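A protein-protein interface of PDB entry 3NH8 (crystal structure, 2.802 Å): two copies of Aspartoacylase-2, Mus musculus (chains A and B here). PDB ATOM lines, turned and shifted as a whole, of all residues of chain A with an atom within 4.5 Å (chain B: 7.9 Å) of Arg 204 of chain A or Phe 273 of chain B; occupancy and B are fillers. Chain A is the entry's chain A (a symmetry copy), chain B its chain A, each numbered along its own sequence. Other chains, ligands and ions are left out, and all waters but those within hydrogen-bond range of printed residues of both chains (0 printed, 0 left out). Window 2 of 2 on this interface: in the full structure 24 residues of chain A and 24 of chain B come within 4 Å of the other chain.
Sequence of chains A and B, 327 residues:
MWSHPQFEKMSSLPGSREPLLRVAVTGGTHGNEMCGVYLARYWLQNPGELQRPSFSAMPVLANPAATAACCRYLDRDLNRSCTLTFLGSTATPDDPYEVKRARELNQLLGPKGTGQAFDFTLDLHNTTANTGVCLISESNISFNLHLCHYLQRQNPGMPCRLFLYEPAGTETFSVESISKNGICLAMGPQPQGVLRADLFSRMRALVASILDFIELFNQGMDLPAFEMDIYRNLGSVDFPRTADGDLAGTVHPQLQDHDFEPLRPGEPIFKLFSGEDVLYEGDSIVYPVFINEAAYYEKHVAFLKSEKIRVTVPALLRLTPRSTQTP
O of Phe 273 of chain B sits at hydrogen-bond distance from NH1 of Arg 204 of chain A (2.9 Å). The side-chain hydroxyl of Thr 250 of chain B lies within hydrogen-bond range of the backbone carbonyl oxygen of Leu 195 of chain A (2.8 Å).
NH2 of Arg 204 of chain A lies within salt-bridge range of OE1 of Glu 49 of chain A (2.7 Å). O of Thr 250 of chain B lies within hydrogen-bond range of N of Lys 271 of chain B. N of Phe 273 of chain B sits at hydrogen-bond distance from O of Ala 248 of chain B (3.0 Å).
Tyr 38 of chain A touches Leu 247 of chain B (CE1 to CB, 3.6 Å). Phe 273 of chain B touches Tyr 42 of chain A (CB to CE1, 3.8 Å). Leu 195 of chain A touches Phe 273 of chain B (CD2 to CZ, 3.95 Å). Phe 200 of chain A touches Phe 273 of chain B.
Phe 273 of chain B touches just these residues of chain A: Tyr 42, Leu 195, Phe 200 and Arg 204. No residue of chain B comes within 4 Å of Ala 205 of chain A. Of the printed residues of chain B, Tyr 38 of chain A touches Leu 247 (3.6 Å). Printed residues of chain A within 4 Å of Leu 247 of chain B: Tyr 38. Of the printed residues of chain B, Phe 200 of chain A touches Phe 273 (3.4 Å). Of the printed residues of chain B, Leu 195 of chain A touches Thr 250 (2.8 Å) and Phe 273 (3.95 Å). The nearest residue of chain B that does not touch Arg 204 of chain A is Ser 274 of chain B (5.1 Å). The nearest printed residue of chain B that does not touch Phe 200 of chain A is Thr 250 of chain B (5.7 Å).
Hydrophobic or aromatic side chains of chain B within 4 Å of the printed part of chain A: Leu 247 and Phe 273. Hydrophobic or aromatic side chains of chain A that line the printed part of chain B: Tyr 38, Tyr 42, Leu 195 and Phe 200. Among the printed residues, 6 pairs touch across the chains.
No position is printed for both chains.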
ATOM      1  N   TYR A  38       0.921  -1.057  32.884  1.00  0.00           N
ATOM      2  CA  TYR A  38      -0.340  -1.422  32.281  1.00  0.00           C
ATOM      3  C   TYR A  38      -0.165  -1.884  30.842  1.00  0.00           C
ATOM      4  O   TYR A  38      -0.954  -2.682  30.341  1.00  0.00           O
ATOM      5  CB  TYR A  38      -1.444  -0.360  32.523  1.00  0.00           C
ATOM      6  CG  TYR A  38      -2.098  -0.565  33.886  1.00  0.00           C
ATOM      7  CD1 TYR A  38      -3.077  -1.531  34.066  1.00  0.00           C
ATOM      8  CD2 TYR A  38      -1.686   0.152  35.005  1.00  0.00           C
ATOM      9  CE1 TYR A  38      -3.656  -1.753  35.304  1.00  0.00           C
ATOM     10  CE2 TYR A  38      -2.257  -0.074  36.257  1.00  0.00           C
ATOM     11  CZ  TYR A  38      -3.243  -1.028  36.397  1.00  0.00           C
ATOM     12  OH  TYR A  38      -3.836  -1.266  37.626  1.00  0.00           O
ATOM     13  N   LEU A  39       0.899  -1.427  30.199  1.00  0.00           N
ATOM     14  CA  LEU A  39       1.223  -1.956  28.877  1.00  0.00           C
ATOM     15  C   LEU A  39       1.647  -3.429  28.996  1.00  0.00           C
ATOM     16  O   LEU A  39       1.145  -4.291  28.274  1.00  0.00           O
ATOM     17  CB  LEU A  39       2.294  -1.103  28.181  1.00  0.00           C
ATOM     18  CG  LEU A  39       1.807   0.247  27.638  1.00  0.00           C
ATOM     19  CD1 LEU A  39       2.953   1.145  27.217  1.00  0.00           C
ATOM     20  CD2 LEU A  39       0.818   0.051  26.506  1.00  0.00           C
ATOM     21  N   TYR A  42      -1.326  -5.600  29.746  1.00  0.00           N
ATOM     22  CA  TYR A  42      -2.191  -5.623  28.588  1.00  0.00           C
ATOM     23  C   TYR A  42      -1.692  -6.633  27.539  1.00  0.00           C
ATOM     24  O   TYR A  42      -2.421  -7.538  27.125  1.00  0.00           O
ATOM     25  CB  TYR A  42      -2.309  -4.220  27.988  1.00  0.00           C
ATOM     26  CG  TYR A  42      -3.258  -4.178  26.837  1.00  0.00           C
ATOM     27  CD1 TYR A  42      -4.632  -4.263  27.045  1.00  0.00           C
ATOM     28  CD2 TYR A  42      -2.790  -4.095  25.538  1.00  0.00           C
ATOM     29  CE1 TYR A  42      -5.518  -4.258  25.985  1.00  0.00           C
ATOM     30  CE2 TYR A  42      -3.665  -4.078  24.457  1.00  0.00           C
ATOM     31  CZ  TYR A  42      -5.030  -4.162  24.687  1.00  0.00           C
ATOM     32  OH  TYR A  42      -5.897  -4.138  23.609  1.00  0.00           O
ATOM     33  N   GLU A  49      -0.085  -7.041  19.010  1.00  0.00           N
ATOM     34  CA  GLU A  49       0.546  -5.831  18.505  1.00  0.00           C
ATOM     35  C   GLU A  49       2.066  -5.846  18.664  1.00  0.00           C
ATOM     36  O   GLU A  49       2.743  -4.912  18.225  1.00  0.00           O
ATOM     37  CB  GLU A  49      -0.082  -4.586  19.148  1.00  0.00           C
ATOM     38  CG  GLU A  49      -0.022  -4.575  20.673  1.00  0.00           C
ATOM     39  CD  GLU A  49      -0.569  -3.294  21.306  1.00  0.00           C
ATOM     40  OE1 GLU A  49      -1.791  -3.041  21.199  1.00  0.00           O
ATOM     41  OE2 GLU A  49       0.225  -2.547  21.926  1.00  0.00           O
ATOM     42  N   LEU A 195      -2.009   6.734  36.212  1.00  0.00           N
ATOM     43  CA  LEU A 195      -1.898   6.412  34.807  1.00  0.00           C
ATOM     44  C   LEU A 195      -2.606   7.491  34.007  1.00  0.00           C
ATOM     45  O   LEU A 195      -3.832   7.668  34.120  1.00  0.00           O
ATOM     46  CB  LEU A 195      -2.520   5.045  34.520  1.00  0.00           C
ATOM     47  CG  LEU A 195      -2.532   4.519  33.081  1.00  0.00           C
ATOM     48  CD1 LEU A 195      -1.135   4.442  32.517  1.00  0.00           C
ATOM     49  CD2 LEU A 195      -3.140   3.171  33.047  1.00  0.00           C
ATOM     50  N   PHE A 200       0.100   6.761  28.418  1.00  0.00           N
ATOM     51  CA  PHE A 200      -0.118   5.379  28.055  1.00  0.00           C
ATOM     52  C   PHE A 200      -0.163   5.246  26.539  1.00  0.00           C
ATOM     53  O   PHE A 200       0.641   4.531  25.944  1.00  0.00           O
ATOM     54  CB  PHE A 200      -1.435   4.911  28.644  1.00  0.00           C
ATOM     55  CG  PHE A 200      -1.798   3.504  28.294  1.00  0.00           C
ATOM     56  CD1 PHE A 200      -1.243   2.436  28.993  1.00  0.00           C
ATOM     57  CD2 PHE A 200      -2.722   3.246  27.276  1.00  0.00           C
ATOM     58  CE1 PHE A 200      -1.596   1.131  28.683  1.00  0.00           C
ATOM     59  CE2 PHE A 200      -3.091   1.940  26.946  1.00  0.00           C
ATOM     60  CZ  PHE A 200      -2.530   0.877  27.654  1.00  0.00           C
ATOM     61  N   SER A 201      -1.079   5.948  25.892  1.00  0.00           N
ATOM     62  CA  SER A 201      -1.208   5.787  24.460  1.00  0.00           C
ATOM     63  C   SER A 201       0.011   6.276  23.658  1.00  0.00           C
ATOM     64  O   SER A 201       0.356   5.675  22.638  1.00  0.00           O
ATOM     65  CB  SER A 201      -2.459   6.469  23.971  1.00  0.00           C
ATOM     66  OG  SER A 201      -2.202   7.840  23.957  1.00  0.00           O
ATOM     67  N   ARG A 202       0.663   7.346  24.100  1.00  0.00           N
ATOM     68  CA  ARG A 202       1.856   7.812  23.395  1.00  0.00           C
ATOM     69  C   ARG A 202       3.025   6.860  23.610  1.00  0.00           C
ATOM     70  O   ARG A 202       3.915   6.764  22.769  1.00  0.00           O
ATOM     71  CB  ARG A 202       2.259   9.246  23.790  1.00  0.00           C
ATOM     72  CG  ARG A 202       3.178   9.943  22.755  1.00  0.00           C
ATOM     73  CD  ARG A 202       3.487  11.425  23.079  1.00  0.00           C
ATOM     74  NE  ARG A 202       2.346  12.346  22.876  1.00  0.00           N
ATOM     75  CZ  ARG A 202       1.509  12.772  23.840  1.00  0.00           C
ATOM     76  NH1 ARG A 202       1.658  12.369  25.096  1.00  0.00           N
ATOM     77  NH2 ARG A 202       0.509  13.610  23.558  1.00  0.00           N
ATOM     78  N   MET A 203       3.046   6.165  24.740  1.00  0.00           N
ATOM     79  CA  MET A 203       4.135   5.225  24.974  1.00  0.00           C
ATOM     80  C   MET A 203       3.908   4.072  24.029  1.00  0.00           C
ATOM     81  O   MET A 203       4.834   3.606  23.338  1.00  0.00           O
ATOM     82  CB  MET A 203       4.166   4.712  26.410  1.00  0.00           C
ATOM     83  CG  MET A 203       5.547   4.288  26.841  1.00  0.00           C
ATOM     84  SD  MET A 203       5.684   3.523  28.466  1.00  0.00           S
ATOM     85  CE  MET A 203       6.970   4.515  29.262  1.00  0.00           C
ATOM     86  N   ARG A 204       2.649   3.643  24.003  1.00  0.00           N
ATOM     87  CA  ARG A 204       2.199   2.538  23.191  1.00  0.00           C
ATOM     88  C   ARG A 204       2.578   2.758  21.719  1.00  0.00           C
ATOM     89  O   ARG A 204       3.074   1.844  21.033  1.00  0.00           O
ATOM     90  CB  ARG A 204       0.684   2.391  23.366  1.00  0.00           C
ATOM     91  CG  ARG A 204       0.116   1.065  22.940  1.00  0.00           C
ATOM     92  CD  ARG A 204      -1.376   1.124  22.926  1.00  0.00           C
ATOM     93  NE  ARG A 204      -1.985  -0.137  22.535  1.00  0.00           N
ATOM     94  CZ  ARG A 204      -3.295  -0.356  22.534  1.00  0.00           C
ATOM     95  NH1 ARG A 204      -4.124   0.606  22.915  1.00  0.00           N
ATOM     96  NH2 ARG A 204      -3.783  -1.533  22.167  1.00  0.00           N
ATOM     97  N   ALA A 205       2.353   3.971  21.237  1.00  0.00           N
ATOM     98  CA  ALA A 205       2.640   4.284  19.848  1.00  0.00           C
ATOM     99  C   ALA A 205       4.148   4.246  19.606  1.00  0.00           C
ATOM    100  O   ALA A 205       4.605   3.748  18.593  1.00  0.00           O
ATOM    101  CB  ALA A 205       2.049   5.646  19.477  1.00  0.00           C
ATOM    102  N   LEU A 206       4.919   4.759  20.555  1.00  0.00           N
ATOM    103  CA  LEU A 206       6.354   4.863  20.401  1.00  0.00           C
ATOM    104  C   LEU A 206       6.970   3.487  20.439  1.00  0.00           C
ATOM    105  O   LEU A 206       7.879   3.181  19.679  1.00  0.00           O
ATOM    106  CB  LEU A 206       6.932   5.726  21.507  1.00  0.00           C
ATOM    107  CG  LEU A 206       6.720   7.247  21.382  1.00  0.00           C
ATOM    108  CD1 LEU A 206       7.180   8.008  22.623  1.00  0.00           C
ATOM    109  CD2 LEU A 206       7.447   7.771  20.151  1.00  0.00           C
ATOM    110  N   VAL A 207       6.447   2.643  21.321  1.00  0.00           N
ATOM    111  CA  VAL A 207       6.785   1.220  21.322  1.00  0.00           C
ATOM    112  C   VAL A 207       6.419   0.518  19.997  1.00  0.00           C
ATOM    113  O   VAL A 207       7.196  -0.246  19.445  1.00  0.00           O
ATOM    114  CB  VAL A 207       6.093   0.496  22.479  1.00  0.00           C
ATOM    115  CG1 VAL A 207       6.298  -1.011  22.352  1.00  0.00           C
ATOM    116  CG2 VAL A 207       6.595   1.042  23.819  1.00  0.00           C
ATOM    117  N   ALA A 208       5.230   0.768  19.484  1.00  0.00           N
ATOM    118  CA  ALA A 208       4.911   0.210  18.191  1.00  0.00           C
ATOM    119  C   ALA A 208       5.994   0.621  17.219  1.00  0.00           C
ATOM    120  O   ALA A 208       6.431  -0.177  16.384  1.00  0.00           O
ATOM    121  CB  ALA A 208       3.556   0.698  17.709  1.00  0.00           C
ATOM    122  N   PHE B 239     -13.099   3.237  38.317  1.00  0.00           N
ATOM    123  CA  PHE B 239     -12.436   3.087  37.037  1.00  0.00           C
ATOM    124  C   PHE B 239     -13.133   1.988  36.313  1.00  0.00           C
ATOM    125  O   PHE B 239     -13.715   1.118  36.947  1.00  0.00           O
ATOM    126  CB  PHE B 239     -10.983   2.682  37.231  1.00  0.00           C
ATOM    127  CG  PHE B 239     -10.091   3.814  37.587  1.00  0.00           C
ATOM    128  CD1 PHE B 239      -9.903   4.172  38.908  1.00  0.00           C
ATOM    129  CD2 PHE B 239      -9.439   4.528  36.602  1.00  0.00           C
ATOM    130  CE1 PHE B 239      -9.082   5.217  39.239  1.00  0.00           C
ATOM    131  CE2 PHE B 239      -8.615   5.579  36.929  1.00  0.00           C
ATOM    132  CZ  PHE B 239      -8.442   5.922  38.251  1.00  0.00           C
ATOM    133  N   PRO B 240     -13.060   2.005  34.979  1.00  0.00           N
ATOM    134  CA  PRO B 240     -13.567   0.899  34.167  1.00  0.00           C
ATOM    135  C   PRO B 240     -12.787  -0.345  34.552  1.00  0.00           C
ATOM    136  O   PRO B 240     -11.570  -0.293  34.501  1.00  0.00           O
ATOM    137  CB  PRO B 240     -13.175   1.315  32.747  1.00  0.00           C
ATOM    138  CG  PRO B 240     -12.863   2.787  32.812  1.00  0.00           C
ATOM    139  CD  PRO B 240     -12.337   3.007  34.177  1.00  0.00           C
ATOM    140  N   THR B 242     -11.782  -4.725  34.540  1.00  0.00           N
ATOM    141  CA  THR B 242     -11.894  -6.106  34.079  1.00  0.00           C
ATOM    142  C   THR B 242     -12.588  -6.909  35.169  1.00  0.00           C
ATOM    143  O   THR B 242     -12.542  -6.532  36.338  1.00  0.00           O
ATOM    144  CB  THR B 242     -10.507  -6.750  33.737  1.00  0.00           C
ATOM    145  OG1 THR B 242      -9.751  -7.042  34.927  1.00  0.00           O
ATOM    146  CG2 THR B 242      -9.724  -5.834  32.835  1.00  0.00           C
ATOM    147  N   ASP B 246      -9.170  -5.547  37.824  1.00  0.00           N
ATOM    148  CA  ASP B 246      -8.059  -4.799  37.239  1.00  0.00           C
ATOM    149  C   ASP B 246      -8.556  -3.579  36.429  1.00  0.00           C
ATOM    150  O   ASP B 246      -9.714  -3.513  36.010  1.00  0.00           O
ATOM    151  CB  ASP B 246      -7.226  -5.727  36.332  1.00  0.00           C
ATOM    152  CG  ASP B 246      -6.190  -6.549  37.103  1.00  0.00           C
ATOM    153  OD1 ASP B 246      -6.459  -6.913  38.270  1.00  0.00           O
ATOM    154  OD2 ASP B 246      -5.105  -6.836  36.532  1.00  0.00           O
ATOM    155  N   LEU B 247      -7.686  -2.604  36.215  1.00  0.00           N
ATOM    156  CA  LEU B 247      -8.060  -1.503  35.351  1.00  0.00           C
ATOM    157  C   LEU B 247      -8.312  -2.004  33.930  1.00  0.00           C
ATOM    158  O   LEU B 247      -7.674  -2.945  33.472  1.00  0.00           O
ATOM    159  CB  LEU B 247      -6.964  -0.438  35.332  1.00  0.00           C
ATOM    160  CG  LEU B 247      -6.861   0.579  36.468  1.00  0.00           C
ATOM    161  CD1 LEU B 247      -6.891   1.962  35.887  1.00  0.00           C
ATOM    162  CD2 LEU B 247      -7.964   0.427  37.500  1.00  0.00           C
ATOM    163  N   ALA B 248      -9.224  -1.360  33.225  1.00  0.00           N
ATOM    164  CA  ALA B 248      -9.490  -1.708  31.847  1.00  0.00           C
ATOM    165  C   ALA B 248      -9.326  -0.447  31.035  1.00  0.00           C
ATOM    166  O   ALA B 248      -9.393  -0.453  29.806  1.00  0.00           O
ATOM    167  CB  ALA B 248     -10.889  -2.252  31.707  1.00  0.00           C
ATOM    168  N   GLY B 249      -9.102   0.651  31.738  1.00  0.00           N
ATOM    169  CA  GLY B 249      -8.833   1.921  31.083  1.00  0.00           C
ATOM    170  C   GLY B 249      -8.538   2.959  32.133  1.00  0.00           C
ATOM    171  O   GLY B 249      -8.514   2.622  33.315  1.00  0.00           O
ATOM    172  N   THR B 250      -8.324   4.202  31.714  1.00  0.00           N
ATOM    173  CA  THR B 250      -8.080   5.291  32.657  1.00  0.00           C
ATOM    174  C   THR B 250      -8.860   6.570  32.345  1.00  0.00           C
ATOM    175  O   THR B 250      -9.612   6.658  31.368  1.00  0.00           O
ATOM    176  CB  THR B 250      -6.578   5.648  32.773  1.00  0.00           C
ATOM    177  OG1 THR B 250      -6.374   6.501  33.910  1.00  0.00           O
ATOM    178  CG2 THR B 250      -6.100   6.352  31.508  1.00  0.00           C
ATOM    179  N   VAL B 251      -8.684   7.562  33.205  1.00  0.00           N
ATOM    180  CA  VAL B 251      -9.411   8.803  33.048  1.00  0.00           C
ATOM    181  C   VAL B 251      -9.149   9.312  31.650  1.00  0.00           C
ATOM    182  O   VAL B 251      -8.001   9.315  31.195  1.00  0.00           O
ATOM    183  CB  VAL B 251      -9.007   9.852  34.095  1.00  0.00           C
ATOM    184  CG1 VAL B 251      -9.590  11.219  33.744  1.00  0.00           C
ATOM    185  CG2 VAL B 251      -9.446   9.389  35.467  1.00  0.00           C
ATOM    186  N   PHE B 270     -13.851   8.170  30.391  1.00  0.00           N
ATOM    187  CA  PHE B 270     -12.780   7.188  30.409  1.00  0.00           C
ATOM    188  C   PHE B 270     -12.310   6.853  29.024  1.00  0.00           C
ATOM    189  O   PHE B 270     -13.024   7.081  28.052  1.00  0.00           O
ATOM    190  CB  PHE B 270     -13.255   5.930  31.098  1.00  0.00           C
ATOM    191  CG  PHE B 270     -13.417   6.104  32.560  1.00  0.00           C
ATOM    192  CD1 PHE B 270     -12.304   6.355  33.360  1.00  0.00           C
ATOM    193  CD2 PHE B 270     -14.677   6.049  33.148  1.00  0.00           C
ATOM    194  CE1 PHE B 270     -12.438   6.518  34.729  1.00  0.00           C
ATOM    195  CE2 PHE B 270     -14.829   6.213  34.525  1.00  0.00           C
ATOM    196  CZ  PHE B 270     -13.708   6.446  35.317  1.00  0.00           C
ATOM    197  N   LYS B 271     -11.090   6.339  28.929  1.00  0.00           N
ATOM    198  CA  LYS B 271     -10.638   5.731  27.684  1.00  0.00           C
ATOM    199  C   LYS B 271     -10.080   4.350  27.958  1.00  0.00           C
ATOM    200  O   LYS B 271      -9.126   4.180  28.716  1.00  0.00           O
ATOM    201  CB  LYS B 271      -9.631   6.601  26.930  1.00  0.00           C
ATOM    202  CG  LYS B 271      -9.289   6.053  25.551  1.00  0.00           C
ATOM    203  CD  LYS B 271      -8.695   7.122  24.652  1.00  0.00           C
ATOM    204  CE  LYS B 271      -9.755   7.762  23.754  1.00  0.00           C
ATOM    205  NZ  LYS B 271     -10.308   6.814  22.720  1.00  0.00           N
ATOM    206  N   LEU B 272     -10.708   3.358  27.343  1.00  0.00           N
ATOM    207  CA  LEU B 272     -10.333   1.974  27.539  1.00  0.00           C
ATOM    208  C   LEU B 272      -9.045   1.665  26.803  1.00  0.00           C
ATOM    209  O   LEU B 272      -8.664   2.346  25.857  1.00  0.00           O
ATOM    210  CB  LEU B 272     -11.464   1.068  27.062  1.00  0.00           C
ATOM    211  CG  LEU B 272     -12.781   1.228  27.832  1.00  0.00           C
ATOM    212  CD1 LEU B 272     -13.715   0.141  27.397  1.00  0.00           C
ATOM    213  CD2 LEU B 272     -12.524   1.115  29.317  1.00  0.00           C
ATOM    214  N   PHE B 273      -8.353   0.641  27.258  1.00  0.00           N
ATOM    215  CA  PHE B 273      -7.138   0.255  26.595  1.00  0.00           C
ATOM    216  C   PHE B 273      -7.439  -0.237  25.169  1.00  0.00           C
ATOM    217  O   PHE B 273      -6.600  -0.157  24.275  1.00  0.00           O
ATOM    218  CB  PHE B 273      -6.442  -0.817  27.416  1.00  0.00           C
ATOM    219  CG  PHE B 273      -6.100  -0.382  28.805  1.00  0.00           C
ATOM    220  CD1 PHE B 273      -5.681   0.908  29.054  1.00  0.00           C
ATOM    221  CD2 PHE B 273      -6.173  -1.261  29.858  1.00  0.00           C
ATOM    222  CE1 PHE B 273      -5.359   1.312  30.335  1.00  0.00           C
ATOM    223  CE2 PHE B 273      -5.845  -0.862  31.149  1.00  0.00           C
ATOM    224  CZ  PHE B 273      -5.444   0.424  31.381  1.00  0.00           C
ATOM    225  N   SER B 274      -8.654  -0.728  24.966  1.00  0.00           N
ATOM    226  CA  SER B 274      -9.070  -1.272  23.684  1.00  0.00           C
ATOM    227  C   SER B 274      -9.400  -0.168  22.697  1.00  0.00           C
ATOM    228  O   SER B 274      -9.766  -0.451  21.550  1.00  0.00           O
ATOM    229  CB  SER B 274     -10.323  -2.102  23.870  1.00  0.00           C
ATOM    230  OG  SER B 274     -11.417  -1.228  24.077  1.00  0.00           O
ATOM    231  N   GLY B 275      -9.311   1.083  23.152  1.00  0.00           N
ATOM    232  CA  GLY B 275      -9.516   2.238  22.287  1.00  0.00           C
ATOM    233  C   GLY B 275     -10.871   2.927  22.386  1.00  0.00           C
ATOM    234  O   GLY B 275     -11.050   4.046  21.896  1.00  0.00           O
ATOM    235  N   GLU B 276     -11.824   2.263  23.027  1.00  0.00           N
ATOM    236  CA  GLU B 276     -13.183   2.792  23.145  1.00  0.00           C
ATOM    237  C   GLU B 276     -13.379   3.859  24.245  1.00  0.00           C
ATOM    238  O   GLU B 276     -13.057   3.610  25.414  1.00  0.00           O
ATOM    239  CB  GLU B 276     -14.144   1.627  23.400  1.00  0.00           C
ATOM    240  CG  GLU B 276     -13.606   0.279  22.906  1.00  0.00           C
ATOM    241  CD  GLU B 276     -14.542  -0.895  23.214  1.00  0.00           C
ATOM    242  OE1 GLU B 276     -15.484  -0.721  24.027  1.00  0.00           O
ATOM    243  OE2 GLU B 276     -14.333  -1.997  22.645  1.00  0.00           O
ATOM    244  N   ASP B 277     -13.920   5.023  23.867  1.00  0.00           N
ATOM    245  CA  ASP B 277     -14.419   6.024  24.824  1.00  0.00           C
ATOM    246  C   ASP B 277     -15.556   5.516  25.737  1.00  0.00           C
ATOM    247  O   ASP B 277     -16.525   4.933  25.269  1.00  0.00           O
ATOM    248  CB  ASP B 277     -14.939   7.248  24.072  1.00  0.00           C
ATOM    249  CG  ASP B 277     -13.827   8.089  23.474  1.00  0.00           C
ATOM    250  OD1 ASP B 277     -12.641   7.711  23.639  1.00  0.00           O
ATOM    251  OD2 ASP B 277     -14.134   9.138  22.844  1.00  0.00           O
